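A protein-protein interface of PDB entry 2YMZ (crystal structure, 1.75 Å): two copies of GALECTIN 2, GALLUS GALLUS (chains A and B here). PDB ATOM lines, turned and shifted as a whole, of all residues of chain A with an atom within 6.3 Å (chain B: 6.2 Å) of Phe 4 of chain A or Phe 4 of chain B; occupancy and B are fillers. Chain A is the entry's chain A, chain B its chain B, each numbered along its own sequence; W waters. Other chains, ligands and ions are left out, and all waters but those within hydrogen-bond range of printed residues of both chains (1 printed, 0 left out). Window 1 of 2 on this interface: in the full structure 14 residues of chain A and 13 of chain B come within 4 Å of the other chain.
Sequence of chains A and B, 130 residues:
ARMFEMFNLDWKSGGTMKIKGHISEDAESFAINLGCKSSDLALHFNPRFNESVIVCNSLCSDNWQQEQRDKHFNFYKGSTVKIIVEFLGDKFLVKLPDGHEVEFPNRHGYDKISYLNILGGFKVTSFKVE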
ATOM      1  N   ALA A   1     -26.923  -2.334 -15.775  1.00  0.00           N
ATOM      2  CA  ALA A   1     -26.909  -3.221 -16.971  1.00  0.00           C
ATOM      3  C   ALA A   1     -26.228  -4.552 -16.628  1.00  0.00           C
ATOM      4  O   ALA A   1     -25.637  -4.716 -15.509  1.00  0.00           O
ATOM      5  CB  ALA A   1     -26.182  -2.558 -18.125  1.00  0.00           C
ATOM      6  N   ARG A   2     -26.359  -5.476 -17.594  1.00  0.00           N
ATOM      7  CA  ARG A   2     -25.690  -6.819 -17.662  1.00  0.00           C
ATOM      8  C   ARG A   2     -24.158  -6.772 -17.587  1.00  0.00           C
ATOM      9  O   ARG A   2     -23.468  -6.328 -18.492  1.00  0.00           O
ATOM     10  CB  ARG A   2     -26.125  -7.511 -18.963  1.00  0.00           C
ATOM     11  CG  ARG A   2     -25.533  -8.874 -19.264  1.00  0.00           C
ATOM     12  CD  ARG A   2     -26.575  -9.716 -19.987  1.00  0.00           C
ATOM     13  NE  ARG A   2     -27.756  -9.916 -19.129  1.00  0.00           N
ATOM     14  CZ  ARG A   2     -28.926 -10.409 -19.538  1.00  0.00           C
ATOM     15  NH1 ARG A   2     -29.113 -10.771 -20.808  1.00  0.00           N
ATOM     16  NH2 ARG A   2     -29.920 -10.547 -18.672  1.00  0.00           N
ATOM     17  N   MET A   3     -23.607  -7.226 -16.485  1.00  0.00           N
ATOM     18  CA  MET A   3     -22.176  -7.144 -16.364  1.00  0.00           C
ATOM     19  C   MET A   3     -21.593  -8.475 -16.959  1.00  0.00           C
ATOM     20  O   MET A   3     -20.710  -8.453 -17.844  1.00  0.00           O
ATOM     21  CB  MET A   3     -21.790  -6.850 -14.886  1.00  0.00           C
ATOM     22  CG  MET A   3     -22.393  -5.493 -14.368  1.00  0.00           C
ATOM     23  SD  MET A   3     -21.764  -4.043 -15.312  1.00  0.00           S
ATOM     24  CE  MET A   3     -20.087  -4.086 -14.701  1.00  0.00           C
ATOM     25  N   PHE A   4     -22.149  -9.603 -16.511  1.00  0.00           N
ATOM     26  CA  PHE A   4     -21.498 -10.888 -16.574  1.00  0.00           C
ATOM     27  C   PHE A   4     -22.633 -11.890 -16.863  1.00  0.00           C
ATOM     28  O   PHE A   4     -23.691 -11.849 -16.234  1.00  0.00           O
ATOM     29  CB  PHE A   4     -20.920 -11.033 -15.182  1.00  0.00           C
ATOM     30  CG  PHE A   4     -20.208 -12.291 -14.868  1.00  0.00           C
ATOM     31  CD1 PHE A   4     -20.895 -13.449 -14.530  1.00  0.00           C
ATOM     32  CD2 PHE A   4     -18.833 -12.271 -14.708  1.00  0.00           C
ATOM     33  CE1 PHE A   4     -20.206 -14.590 -14.166  1.00  0.00           C
ATOM     34  CE2 PHE A   4     -18.143 -13.433 -14.339  1.00  0.00           C
ATOM     35  CZ  PHE A   4     -18.846 -14.587 -14.072  1.00  0.00           C
ATOM     36  N   GLU A   5     -22.443 -12.806 -17.791  1.00  0.00           N
ATOM     37  CA  GLU A   5     -23.468 -13.824 -17.954  1.00  0.00           C
ATOM     38  C   GLU A   5     -22.716 -15.120 -18.287  1.00  0.00           C
ATOM     39  O   GLU A   5     -21.713 -15.082 -19.023  1.00  0.00           O
ATOM     40  CB  GLU A   5     -24.363 -13.366 -19.113  1.00  0.00           C
ATOM     41  CG  GLU A   5     -25.632 -14.151 -19.240  1.00  0.00           C
ATOM     42  CD  GLU A   5     -26.630 -13.521 -20.256  1.00  0.00           C
ATOM     43  OE1 GLU A   5     -26.186 -12.944 -21.273  1.00  0.00           O
ATOM     44  OE2 GLU A   5     -27.832 -13.663 -20.022  1.00  0.00           O
ATOM     45  N   MET A   6     -23.165 -16.203 -17.695  1.00  0.00           N
ATOM     46  CA  MET A   6     -22.528 -17.508 -17.954  1.00  0.00           C
ATOM     47  C   MET A   6     -23.640 -18.559 -18.180  1.00  0.00           C
ATOM     48  O   MET A   6     -24.657 -18.542 -17.495  1.00  0.00           O
ATOM     49  CB  MET A   6     -21.526 -17.797 -16.816  1.00  0.00           C
ATOM     50  CG  MET A   6     -21.038 -19.212 -16.667  1.00  0.00           C
ATOM     51  SD  MET A   6     -19.636 -19.091 -15.520  1.00  0.00           S
ATOM     52  CE  MET A   6     -18.874 -20.657 -15.959  1.00  0.00           C
ATOM     53  N   PHE A   7     -23.411 -19.476 -19.137  1.00  0.00           N
ATOM     54  CA  PHE A   7     -24.423 -20.452 -19.546  1.00  0.00           C
ATOM     55  C   PHE A   7     -23.837 -21.858 -19.319  1.00  0.00           C
ATOM     56  O   PHE A   7     -22.623 -22.017 -19.083  1.00  0.00           O
ATOM     57  CB  PHE A   7     -24.809 -20.276 -21.016  1.00  0.00           C
ATOM     58  CG  PHE A   7     -25.293 -18.898 -21.362  1.00  0.00           C
ATOM     59  CD1 PHE A   7     -24.386 -17.914 -21.760  1.00  0.00           C
ATOM     60  CD2 PHE A   7     -26.639 -18.580 -21.263  1.00  0.00           C
ATOM     61  CE1 PHE A   7     -24.819 -16.623 -22.044  1.00  0.00           C
ATOM     62  CE2 PHE A   7     -27.080 -17.269 -21.570  1.00  0.00           C
ATOM     63  CZ  PHE A   7     -26.180 -16.311 -21.978  1.00  0.00           C
ATOM     64  N   TYR A 115     -27.314 -21.387 -15.264  1.00  0.00           N
ATOM     65  CA  TYR A 115     -27.168 -20.079 -15.762  1.00  0.00           C
ATOM     66  C   TYR A 115     -26.862 -19.097 -14.577  1.00  0.00           C
ATOM     67  O   TYR A 115     -27.451 -19.228 -13.499  1.00  0.00           O
ATOM     68  CB  TYR A 115     -28.531 -19.674 -16.340  1.00  0.00           C
ATOM     69  CG  TYR A 115     -28.634 -18.246 -16.747  1.00  0.00           C
ATOM     70  CD1 TYR A 115     -28.124 -17.806 -17.952  1.00  0.00           C
ATOM     71  CD2 TYR A 115     -29.281 -17.328 -15.897  1.00  0.00           C
ATOM     72  CE1 TYR A 115     -28.176 -16.486 -18.295  1.00  0.00           C
ATOM     73  CE2 TYR A 115     -29.355 -15.975 -16.227  1.00  0.00           C
ATOM     74  CZ  TYR A 115     -28.824 -15.567 -17.412  1.00  0.00           C
ATOM     75  OH  TYR A 115     -28.985 -14.241 -17.805  1.00  0.00           O
ATOM     76  N   LEU A 116     -25.953 -18.133 -14.847  1.00  0.00           N
ATOM     77  CA  LEU A 116     -25.652 -17.068 -13.866  1.00  0.00           C
ATOM     78  C   LEU A 116     -25.631 -15.712 -14.600  1.00  0.00           C
ATOM     79  O   LEU A 116     -25.072 -15.586 -15.678  1.00  0.00           O
ATOM     80  CB  LEU A 116     -24.222 -17.324 -13.335  1.00  0.00           C
ATOM     81  CG  LEU A 116     -23.438 -16.238 -12.543  1.00  0.00           C
ATOM     82  CD1 LEU A 116     -24.132 -15.808 -11.251  1.00  0.00           C
ATOM     83  CD2 LEU A 116     -22.014 -16.769 -12.241  1.00  0.00           C
ATOM     84  N   ASN A 117     -26.146 -14.645 -13.966  1.00  0.00           N
ATOM     85  CA  ASN A 117     -25.805 -13.348 -14.488  1.00  0.00           C
ATOM     86  C   ASN A 117     -25.599 -12.427 -13.255  1.00  0.00           C
ATOM     87  O   ASN A 117     -25.995 -12.778 -12.117  1.00  0.00           O
ATOM     88  CB  ASN A 117     -26.824 -12.823 -15.514  1.00  0.00           C
ATOM     89  CG  ASN A 117     -28.112 -12.322 -14.917  1.00  0.00           C
ATOM     90  OD1 ASN A 117     -28.122 -11.664 -13.880  1.00  0.00           O
ATOM     91  ND2 ASN A 117     -29.225 -12.545 -15.639  1.00  0.00           N
ATOM     92  N   ILE A 118     -24.797 -11.394 -13.482  1.00  0.00           N
ATOM     93  CA  ILE A 118     -24.580 -10.432 -12.402  1.00  0.00           C
ATOM     94  C   ILE A 118     -24.943  -9.107 -13.048  1.00  0.00           C
ATOM     95  O   ILE A 118     -24.484  -8.840 -14.154  1.00  0.00           O
ATOM     96  CB  ILE A 118     -23.123 -10.514 -11.905  1.00  0.00           C
ATOM     97  CG1 ILE A 118     -22.997 -11.796 -11.099  1.00  0.00           C
ATOM     98  CG2 ILE A 118     -22.985  -9.399 -10.815  1.00  0.00           C
ATOM     99  CD1 ILE A 118     -21.622 -12.274 -10.718  1.00  0.00           C
ATOM    100  N   LEU A 119     -25.771  -8.284 -12.381  1.00  0.00           N
ATOM    101  CA  LEU A 119     -26.289  -7.042 -12.995  1.00  0.00           C
ATOM    102  C   LEU A 119     -26.076  -5.899 -11.983  1.00  0.00           C
ATOM    103  O   LEU A 119     -25.970  -6.165 -10.748  1.00  0.00           O
ATOM    104  CB  LEU A 119     -27.812  -7.131 -13.191  1.00  0.00           C
ATOM    105  CG  LEU A 119     -28.419  -8.311 -14.006  1.00  0.00           C
ATOM    106  CD1 LEU A 119     -29.911  -8.145 -14.285  1.00  0.00           C
ATOM    107  CD2 LEU A 119     -27.669  -8.402 -15.308  1.00  0.00           C
ATOM    108  N   VAL A 124     -17.230  -7.760 -11.663  1.00  0.00           N
ATOM    109  CA  VAL A 124     -16.591  -8.969 -11.176  1.00  0.00           C
ATOM    110  C   VAL A 124     -15.065  -8.910 -11.365  1.00  0.00           C
ATOM    111  O   VAL A 124     -14.559  -8.600 -12.447  1.00  0.00           O
ATOM    112  CB  VAL A 124     -17.178 -10.235 -11.906  1.00  0.00           C
ATOM    113  CG1 VAL A 124     -16.413 -11.506 -11.516  1.00  0.00           C
ATOM    114  CG2 VAL A 124     -18.674 -10.349 -11.552  1.00  0.00           C
ATOM    115  N   PHE A 127     -13.927 -15.044 -10.019  1.00  0.00           N
ATOM    116  CA  PHE A 127     -15.096 -15.920  -9.975  1.00  0.00           C
ATOM    117  C   PHE A 127     -14.529 -17.330  -9.877  1.00  0.00           C
ATOM    118  O   PHE A 127     -13.617 -17.653 -10.619  1.00  0.00           O
ATOM    119  CB  PHE A 127     -15.895 -15.750 -11.267  1.00  0.00           C
ATOM    120  CG  PHE A 127     -16.887 -16.841 -11.510  1.00  0.00           C
ATOM    121  CD1 PHE A 127     -18.140 -16.813 -10.873  1.00  0.00           C
ATOM    122  CD2 PHE A 127     -16.565 -17.899 -12.391  1.00  0.00           C
ATOM    123  CE1 PHE A 127     -19.062 -17.881 -11.091  1.00  0.00           C
ATOM    124  CE2 PHE A 127     -17.468 -18.923 -12.591  1.00  0.00           C
ATOM    125  CZ  PHE A 127     -18.718 -18.895 -11.972  1.00  0.00           C
ATOM    126  N   ALA B   1     -23.427 -22.156 -28.039  1.00  0.00           N
ATOM    127  CA  ALA B   1     -21.945 -22.174 -28.129  1.00  0.00           C
ATOM    128  C   ALA B   1     -21.415 -21.086 -27.197  1.00  0.00           C
ATOM    129  O   ALA B   1     -20.348 -21.267 -26.710  1.00  0.00           O
ATOM    130  CB  ALA B   1     -21.430 -21.944 -29.546  1.00  0.00           C
ATOM    131  N   ARG B   2     -22.142 -19.979 -26.952  1.00  0.00           N
ATOM    132  CA  ARG B   2     -21.667 -18.927 -25.969  1.00  0.00           C
ATOM    133  C   ARG B   2     -21.671 -19.437 -24.504  1.00  0.00           C
ATOM    134  O   ARG B   2     -22.663 -19.942 -23.982  1.00  0.00           O
ATOM    135  CB  ARG B   2     -22.449 -17.594 -26.142  1.00  0.00           C
ATOM    136  CG  ARG B   2     -21.864 -16.367 -25.441  1.00  0.00           C
ATOM    137  CD  ARG B   2     -22.827 -15.177 -25.524  1.00  0.00           C
ATOM    138  NE  ARG B   2     -24.232 -15.590 -25.723  1.00  0.00           N
ATOM    139  CZ  ARG B   2     -25.299 -14.934 -25.240  1.00  0.00           C
ATOM    140  NH1 ARG B   2     -25.148 -13.830 -24.525  1.00  0.00           N
ATOM    141  NH2 ARG B   2     -26.524 -15.393 -25.455  1.00  0.00           N
ATOM    142  N   MET B   3     -20.541 -19.375 -23.822  1.00  0.00           N
ATOM    143  CA  MET B   3     -20.488 -20.006 -22.554  1.00  0.00           C
ATOM    144  C   MET B   3     -20.395 -18.877 -21.472  1.00  0.00           C
ATOM    145  O   MET B   3     -20.820 -19.086 -20.343  1.00  0.00           O
ATOM    146  CB  MET B   3     -19.230 -20.865 -22.462  1.00  0.00           C
ATOM    147  CG  MET B   3     -19.211 -21.975 -23.524  1.00  0.00           C
ATOM    148  SD  MET B   3     -20.489 -23.234 -23.178  1.00  0.00           S
ATOM    149  CE  MET B   3     -19.839 -23.925 -21.637  1.00  0.00           C
ATOM    150  N   PHE B   4     -19.720 -17.786 -21.808  1.00  0.00           N
ATOM    151  CA  PHE B   4     -19.332 -16.829 -20.749  1.00  0.00           C
ATOM    152  C   PHE B   4     -19.269 -15.492 -21.494  1.00  0.00           C
ATOM    153  O   PHE B   4     -18.716 -15.415 -22.574  1.00  0.00           O
ATOM    154  CB  PHE B   4     -17.968 -17.254 -20.263  1.00  0.00           C
ATOM    155  CG  PHE B   4     -17.440 -16.558 -19.030  1.00  0.00           C
ATOM    156  CD1 PHE B   4     -17.653 -17.159 -17.759  1.00  0.00           C
ATOM    157  CD2 PHE B   4     -16.493 -15.557 -19.134  1.00  0.00           C
ATOM    158  CE1 PHE B   4     -17.097 -16.596 -16.591  1.00  0.00           C
ATOM    159  CE2 PHE B   4     -15.943 -14.968 -18.004  1.00  0.00           C
ATOM    160  CZ  PHE B   4     -16.236 -15.484 -16.739  1.00  0.00           C
ATOM    161  N   GLU B   5     -19.860 -14.421 -20.952  1.00  0.00           N
ATOM    162  CA  GLU B   5     -19.671 -13.127 -21.677  1.00  0.00           C
ATOM    163  C   GLU B   5     -19.645 -12.035 -20.605  1.00  0.00           C
ATOM    164  O   GLU B   5     -20.394 -12.119 -19.613  1.00  0.00           O
ATOM    165  CB  GLU B   5     -20.863 -12.910 -22.630  1.00  0.00           C
ATOM    166  CG  GLU B   5     -20.785 -11.673 -23.516  1.00  0.00           C
ATOM    167  CD  GLU B   5     -21.917 -11.658 -24.583  1.00  0.00           C
ATOM    168  OE1 GLU B   5     -23.075 -11.972 -24.249  1.00  0.00           O
ATOM    169  OE2 GLU B   5     -21.644 -11.299 -25.717  1.00  0.00           O
ATOM    170  N   MET B   6     -18.710 -11.089 -20.753  1.00  0.00           N
ATOM    171  CA  MET B   6     -18.600  -9.991 -19.835  1.00  0.00           C
ATOM    172  C   MET B   6     -18.467  -8.689 -20.590  1.00  0.00           C
ATOM    173  O   MET B   6     -17.800  -8.620 -21.630  1.00  0.00           O
ATOM    174  CB  MET B   6     -17.365 -10.228 -18.962  1.00  0.00           C
ATOM    175  CG  MET B   6     -17.380  -9.434 -17.712  1.00  0.00           C
ATOM    176  SD  MET B   6     -15.922  -9.981 -16.850  1.00  0.00           S
ATOM    177  CE  MET B   6     -16.217 -11.701 -16.406  1.00  0.00           C
ATOM    178  N   PHE B   7     -19.093  -7.642 -20.042  1.00  0.00           N
ATOM    179  CA  PHE B   7     -19.075  -6.344 -20.665  1.00  0.00           C
ATOM    180  C   PHE B   7     -18.474  -5.388 -19.638  1.00  0.00           C
ATOM    181  O   PHE B   7     -18.260  -5.736 -18.480  1.00  0.00           O
ATOM    182  CB  PHE B   7     -20.509  -5.900 -21.005  1.00  0.00           C
ATOM    183  CG  PHE B   7     -21.229  -6.787 -22.000  1.00  0.00           C
ATOM    184  CD1 PHE B   7     -21.985  -7.877 -21.568  1.00  0.00           C
ATOM    185  CD2 PHE B   7     -21.169  -6.512 -23.353  1.00  0.00           C
ATOM    186  CE1 PHE B   7     -22.671  -8.682 -22.472  1.00  0.00           C
ATOM    187  CE2 PHE B   7     -21.875  -7.319 -24.272  1.00  0.00           C
ATOM    188  CZ  PHE B   7     -22.622  -8.393 -23.823  1.00  0.00           C
ATOM    189  N   TYR B 115     -14.679  -6.063 -23.284  1.00  0.00           N
ATOM    190  CA  TYR B 115     -15.564  -7.125 -23.676  1.00  0.00           C
ATOM    191  C   TYR B 115     -14.739  -8.433 -23.711  1.00  0.00           C
ATOM    192  O   TYR B 115     -13.639  -8.484 -24.249  1.00  0.00           O
ATOM    193  CB  TYR B 115     -16.070  -6.834 -25.099  1.00  0.00           C
ATOM    194  CG  TYR B 115     -16.910  -7.959 -25.601  1.00  0.00           C
ATOM    195  CD1 TYR B 115     -18.204  -8.100 -25.139  1.00  0.00           C
ATOM    196  CD2 TYR B 115     -16.370  -8.930 -26.430  1.00  0.00           C
ATOM    197  CE1 TYR B 115     -19.011  -9.134 -25.553  1.00  0.00           C
ATOM    198  CE2 TYR B 115     -17.172 -10.015 -26.855  1.00  0.00           C
ATOM    199  CZ  TYR B 115     -18.469 -10.087 -26.431  1.00  0.00           C
ATOM    200  OH  TYR B 115     -19.273 -11.136 -26.865  1.00  0.00           O
ATOM    201  N   LEU B 116     -15.289  -9.464 -23.121  1.00  0.00           N
ATOM    202  CA  LEU B 116     -14.673 -10.834 -23.166  1.00  0.00           C
ATOM    203  C   LEU B 116     -15.859 -11.832 -23.471  1.00  0.00           C
ATOM    204  O   LEU B 116     -16.944 -11.716 -22.906  1.00  0.00           O
ATOM    205  CB  LEU B 116     -14.214 -11.211 -21.737  1.00  0.00           C
ATOM    206  CG  LEU B 116     -13.834 -12.719 -21.446  1.00  0.00           C
ATOM    207  CD1 LEU B 116     -12.724 -13.309 -22.335  1.00  0.00           C
ATOM    208  CD2 LEU B 116     -13.486 -12.944 -19.989  1.00  0.00           C
ATOM    209  N   ASN B 117     -15.612 -12.829 -24.338  1.00  0.00           N
ATOM    210  CA  ASN B 117     -16.521 -13.979 -24.319  1.00  0.00           C
ATOM    211  C   ASN B 117     -15.717 -15.235 -24.493  1.00  0.00           C
ATOM    212  O   ASN B 117     -14.597 -15.186 -24.941  1.00  0.00           O
ATOM    213  CB  ASN B 117     -17.665 -13.846 -25.344  1.00  0.00           C
ATOM    214  CG  ASN B 117     -17.222 -14.095 -26.758  1.00  0.00           C
ATOM    215  OD1 ASN B 117     -16.498 -15.039 -27.003  1.00  0.00           O
ATOM    216  ND2 ASN B 117     -17.697 -13.293 -27.698  1.00  0.00           N
ATOM    217  N   ILE B 118     -16.274 -16.318 -24.021  1.00  0.00           N
ATOM    218  CA  ILE B 118     -15.652 -17.600 -24.261  1.00  0.00           C
ATOM    219  C   ILE B 118     -16.735 -18.452 -24.911  1.00  0.00           C
ATOM    220  O   ILE B 118     -17.864 -18.498 -24.417  1.00  0.00           O
ATOM    221  CB  ILE B 118     -15.320 -18.265 -22.931  1.00  0.00           C
ATOM    222  CG1 ILE B 118     -14.223 -17.447 -22.300  1.00  0.00           C
ATOM    223  CG2 ILE B 118     -14.782 -19.701 -23.206  1.00  0.00           C
ATOM    224  CD1 ILE B 118     -13.713 -17.876 -20.949  1.00  0.00           C
ATOM    225  N   LEU B 119     -16.345 -19.137 -25.973  1.00  0.00           N
ATOM    226  CA  LEU B 119     -17.296 -19.943 -26.821  1.00  0.00           C
ATOM    227  C   LEU B 119     -16.789 -21.378 -26.871  1.00  0.00           C
ATOM    228  O   LEU B 119     -15.583 -21.662 -26.728  1.00  0.00           O
ATOM    229  CB  LEU B 119     -17.333 -19.388 -28.245  1.00  0.00           C
ATOM    230  CG  LEU B 119     -17.661 -17.882 -28.385  1.00  0.00           C
ATOM    231  CD1 LEU B 119     -17.592 -17.440 -29.852  1.00  0.00           C
ATOM    232  CD2 LEU B 119     -18.971 -17.609 -27.707  1.00  0.00           C
ATOM    233  N   VAL B 124     -15.716 -22.351 -17.873  1.00  0.00           N
ATOM    234  CA  VAL B 124     -14.878 -21.659 -16.840  1.00  0.00           C
ATOM    235  C   VAL B 124     -15.132 -22.188 -15.431  1.00  0.00           C
ATOM    236  O   VAL B 124     -16.291 -22.303 -14.881  1.00  0.00           O
ATOM    237  CB  VAL B 124     -15.120 -20.127 -16.887  1.00  0.00           C
ATOM    238  CG1 VAL B 124     -14.326 -19.418 -15.761  1.00  0.00           C
ATOM    239  CG2 VAL B 124     -14.710 -19.615 -18.223  1.00  0.00           C
ATOM    240  N   PHE B 127     -11.901 -17.612 -12.790  1.00  0.00           N
ATOM    241  CA  PHE B 127     -11.579 -16.440 -13.656  1.00  0.00           C
ATOM    242  C   PHE B 127     -11.062 -15.347 -12.713  1.00  0.00           C
ATOM    243  O   PHE B 127     -11.674 -15.099 -11.659  1.00  0.00           O
ATOM    244  CB  PHE B 127     -12.909 -15.918 -14.259  1.00  0.00           C
ATOM    245  CG  PHE B 127     -12.787 -14.565 -14.925  1.00  0.00           C
ATOM    246  CD1 PHE B 127     -12.054 -14.412 -16.084  1.00  0.00           C
ATOM    247  CD2 PHE B 127     -13.367 -13.454 -14.322  1.00  0.00           C
ATOM    248  CE1 PHE B 127     -12.000 -13.159 -16.724  1.00  0.00           C
ATOM    249  CE2 PHE B 127     -13.217 -12.190 -14.905  1.00  0.00           C
ATOM    250  CZ  PHE B 127     -12.579 -12.061 -16.117  1.00  0.00           C
HETATM  251  O   HOH W   1     -19.869 -22.091 -18.923  1.00  0.00           O
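The backbone NH (N) of Phe 7 of chain B is in hydrogen-bond range of the backbone carbonyl oxygen (O) of Met 3 of chain A (2.8 Å). The side-chain carboxylate of Glu 5 of chain A lies within salt-bridge range of the guanidinium group of Arg 2 of chain B (3.5 Å). The backbone NH (N) of Glu 5 of chain B sits at hydrogen-bond distance from the backbone carbonyl oxygen (O) of Glu 5 of chain A (2.8 Å). The backbone NH of Phe 7 of chain A is in hydrogen-bond range of the backbone carbonyl oxygen of Met 3 of chain B (2.9 Å). The backbone NH (N) of Phe 127 of chain B sits at hydrogen-bond distance from the backbone carbonyl oxygen (O) of Phe 127 of chain A, 2.8 Å away.
The backbone NH (N) of Met 3 of chain A lies within hydrogen-bond range of the backbone carbonyl oxygen (O) of Ile 118 of chain A (3.0 Å). The backbone carbonyl oxygen (O) of Phe 4 of chain A sits at hydrogen-bond distance from the backbone NH (N) of Ile 118 of chain A (3.0 Å). OE2 of Glu 5 of chain A sits at hydrogen-bond distance from OH of Tyr 115 of chain A. The backbone NH of Met 3 of chain B sits at hydrogen-bond distance from the backbone carbonyl oxygen of Ile 118 of chain B (2.9 Å). The side-chain hydroxyl (OH) of Tyr 115 of chain B lies within hydrogen-bond range of the side-chain carboxylate (OE2) of Glu 5 of chain B (2.6 Å). The backbone NH (N) of Met 6 of chain B sits at hydrogen-bond distance from the backbone carbonyl oxygen (O) of Leu 116 of chain B, at 2.9 Å.
Among the printed residues, merely in contact across the chains: Arg 2 of chain A with Phe 7 of chain B (3.7 Å), Met 3 of chain A with Met 6 of chain B (3.3 Å), Phe 4 of chain A with Phe 4 of chain B (3.7 Å), Phe 4 of chain A with Glu 5 of chain B (3.5 Å), Phe 4 of chain A with Met 6 of chain B (3.2 Å), Glu 5 of chain A with Phe 4 of chain B (3.4 Å), Met 6 of chain A with Met 3 of chain B (3.3 Å), Met 6 of chain A with Phe 4 of chain B (3.6 Å), Met 6 of chain A with Val 124 of chain B (3.2 Å) and Phe 7 of chain A with Arg 2 of chain B (3.5 Å).
Leu 119 of chain A touches none of the printed residues of chain B. Of the printed residues of chain B, Phe 127 of chain A touches Phe 127 (2.8 Å). Of the printed residues of chain A, Phe 4 of chain B touches Phe 4, Glu 5 and Met 6. Printed residues of chain A within 4 Å of Glu 5 of chain B: Phe 4 (3.5 Å) and Glu 5 (2.8 Å). Of the printed residues of chain A, Met 6 of chain B touches Met 3 (3.3 Å) and Phe 4 (3.2 Å). Of the printed residues of chain A, Phe 127 of chain B touches Phe 127 (2.8 Å). The nearest printed residue of chain B that does not touch Phe 4 of chain A is Phe 127 of chain B (4.8 Å). The nearest residue of chain A that does not touch Phe 4 of chain B is Phe 127 of chain A (4.4 Å). The nearest printed residue of chain B that does not touch Arg 2 of chain A is Met 6 of chain B (5.9 Å).
Printed residues of chain A that touch a printed residue of chain B: Arg 2, Met 3, Phe 4, Glu 5, Met 6, Phe 7 and Phe 127. Along chain A the printed residues that touch a printed residue of chain B span positions 2 to 127. Among the printed residues, Asp or Glu carboxylates within 4 Å of a Lys or Arg side-chain nitrogen of the other chain: Glu 5 of chain A with Arg 2 of chain B (3.5 Å).
Met 3 of chain A touches Met 6 of chain B, and with the chains exchanged Met 6 of chain A touches Met 3 of chain B. Met 3 of chain A touches Phe 7 of chain B, and with the chains exchanged Phe 7 of chain A touches Met 3 of chain B. Phe 4 of chain A touches Glu 5 of chain B, and with the chains exchanged Glu 5 of chain A touches Phe 4 of chain B. Phe 127 of chain A touches its own counterpart, Phe 127 of chain B.
Water W1 bridges the backbone carbonyl oxygen of Phe 7 of chain A and the backbone carbonyl oxygen of Met 3 of chain B.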
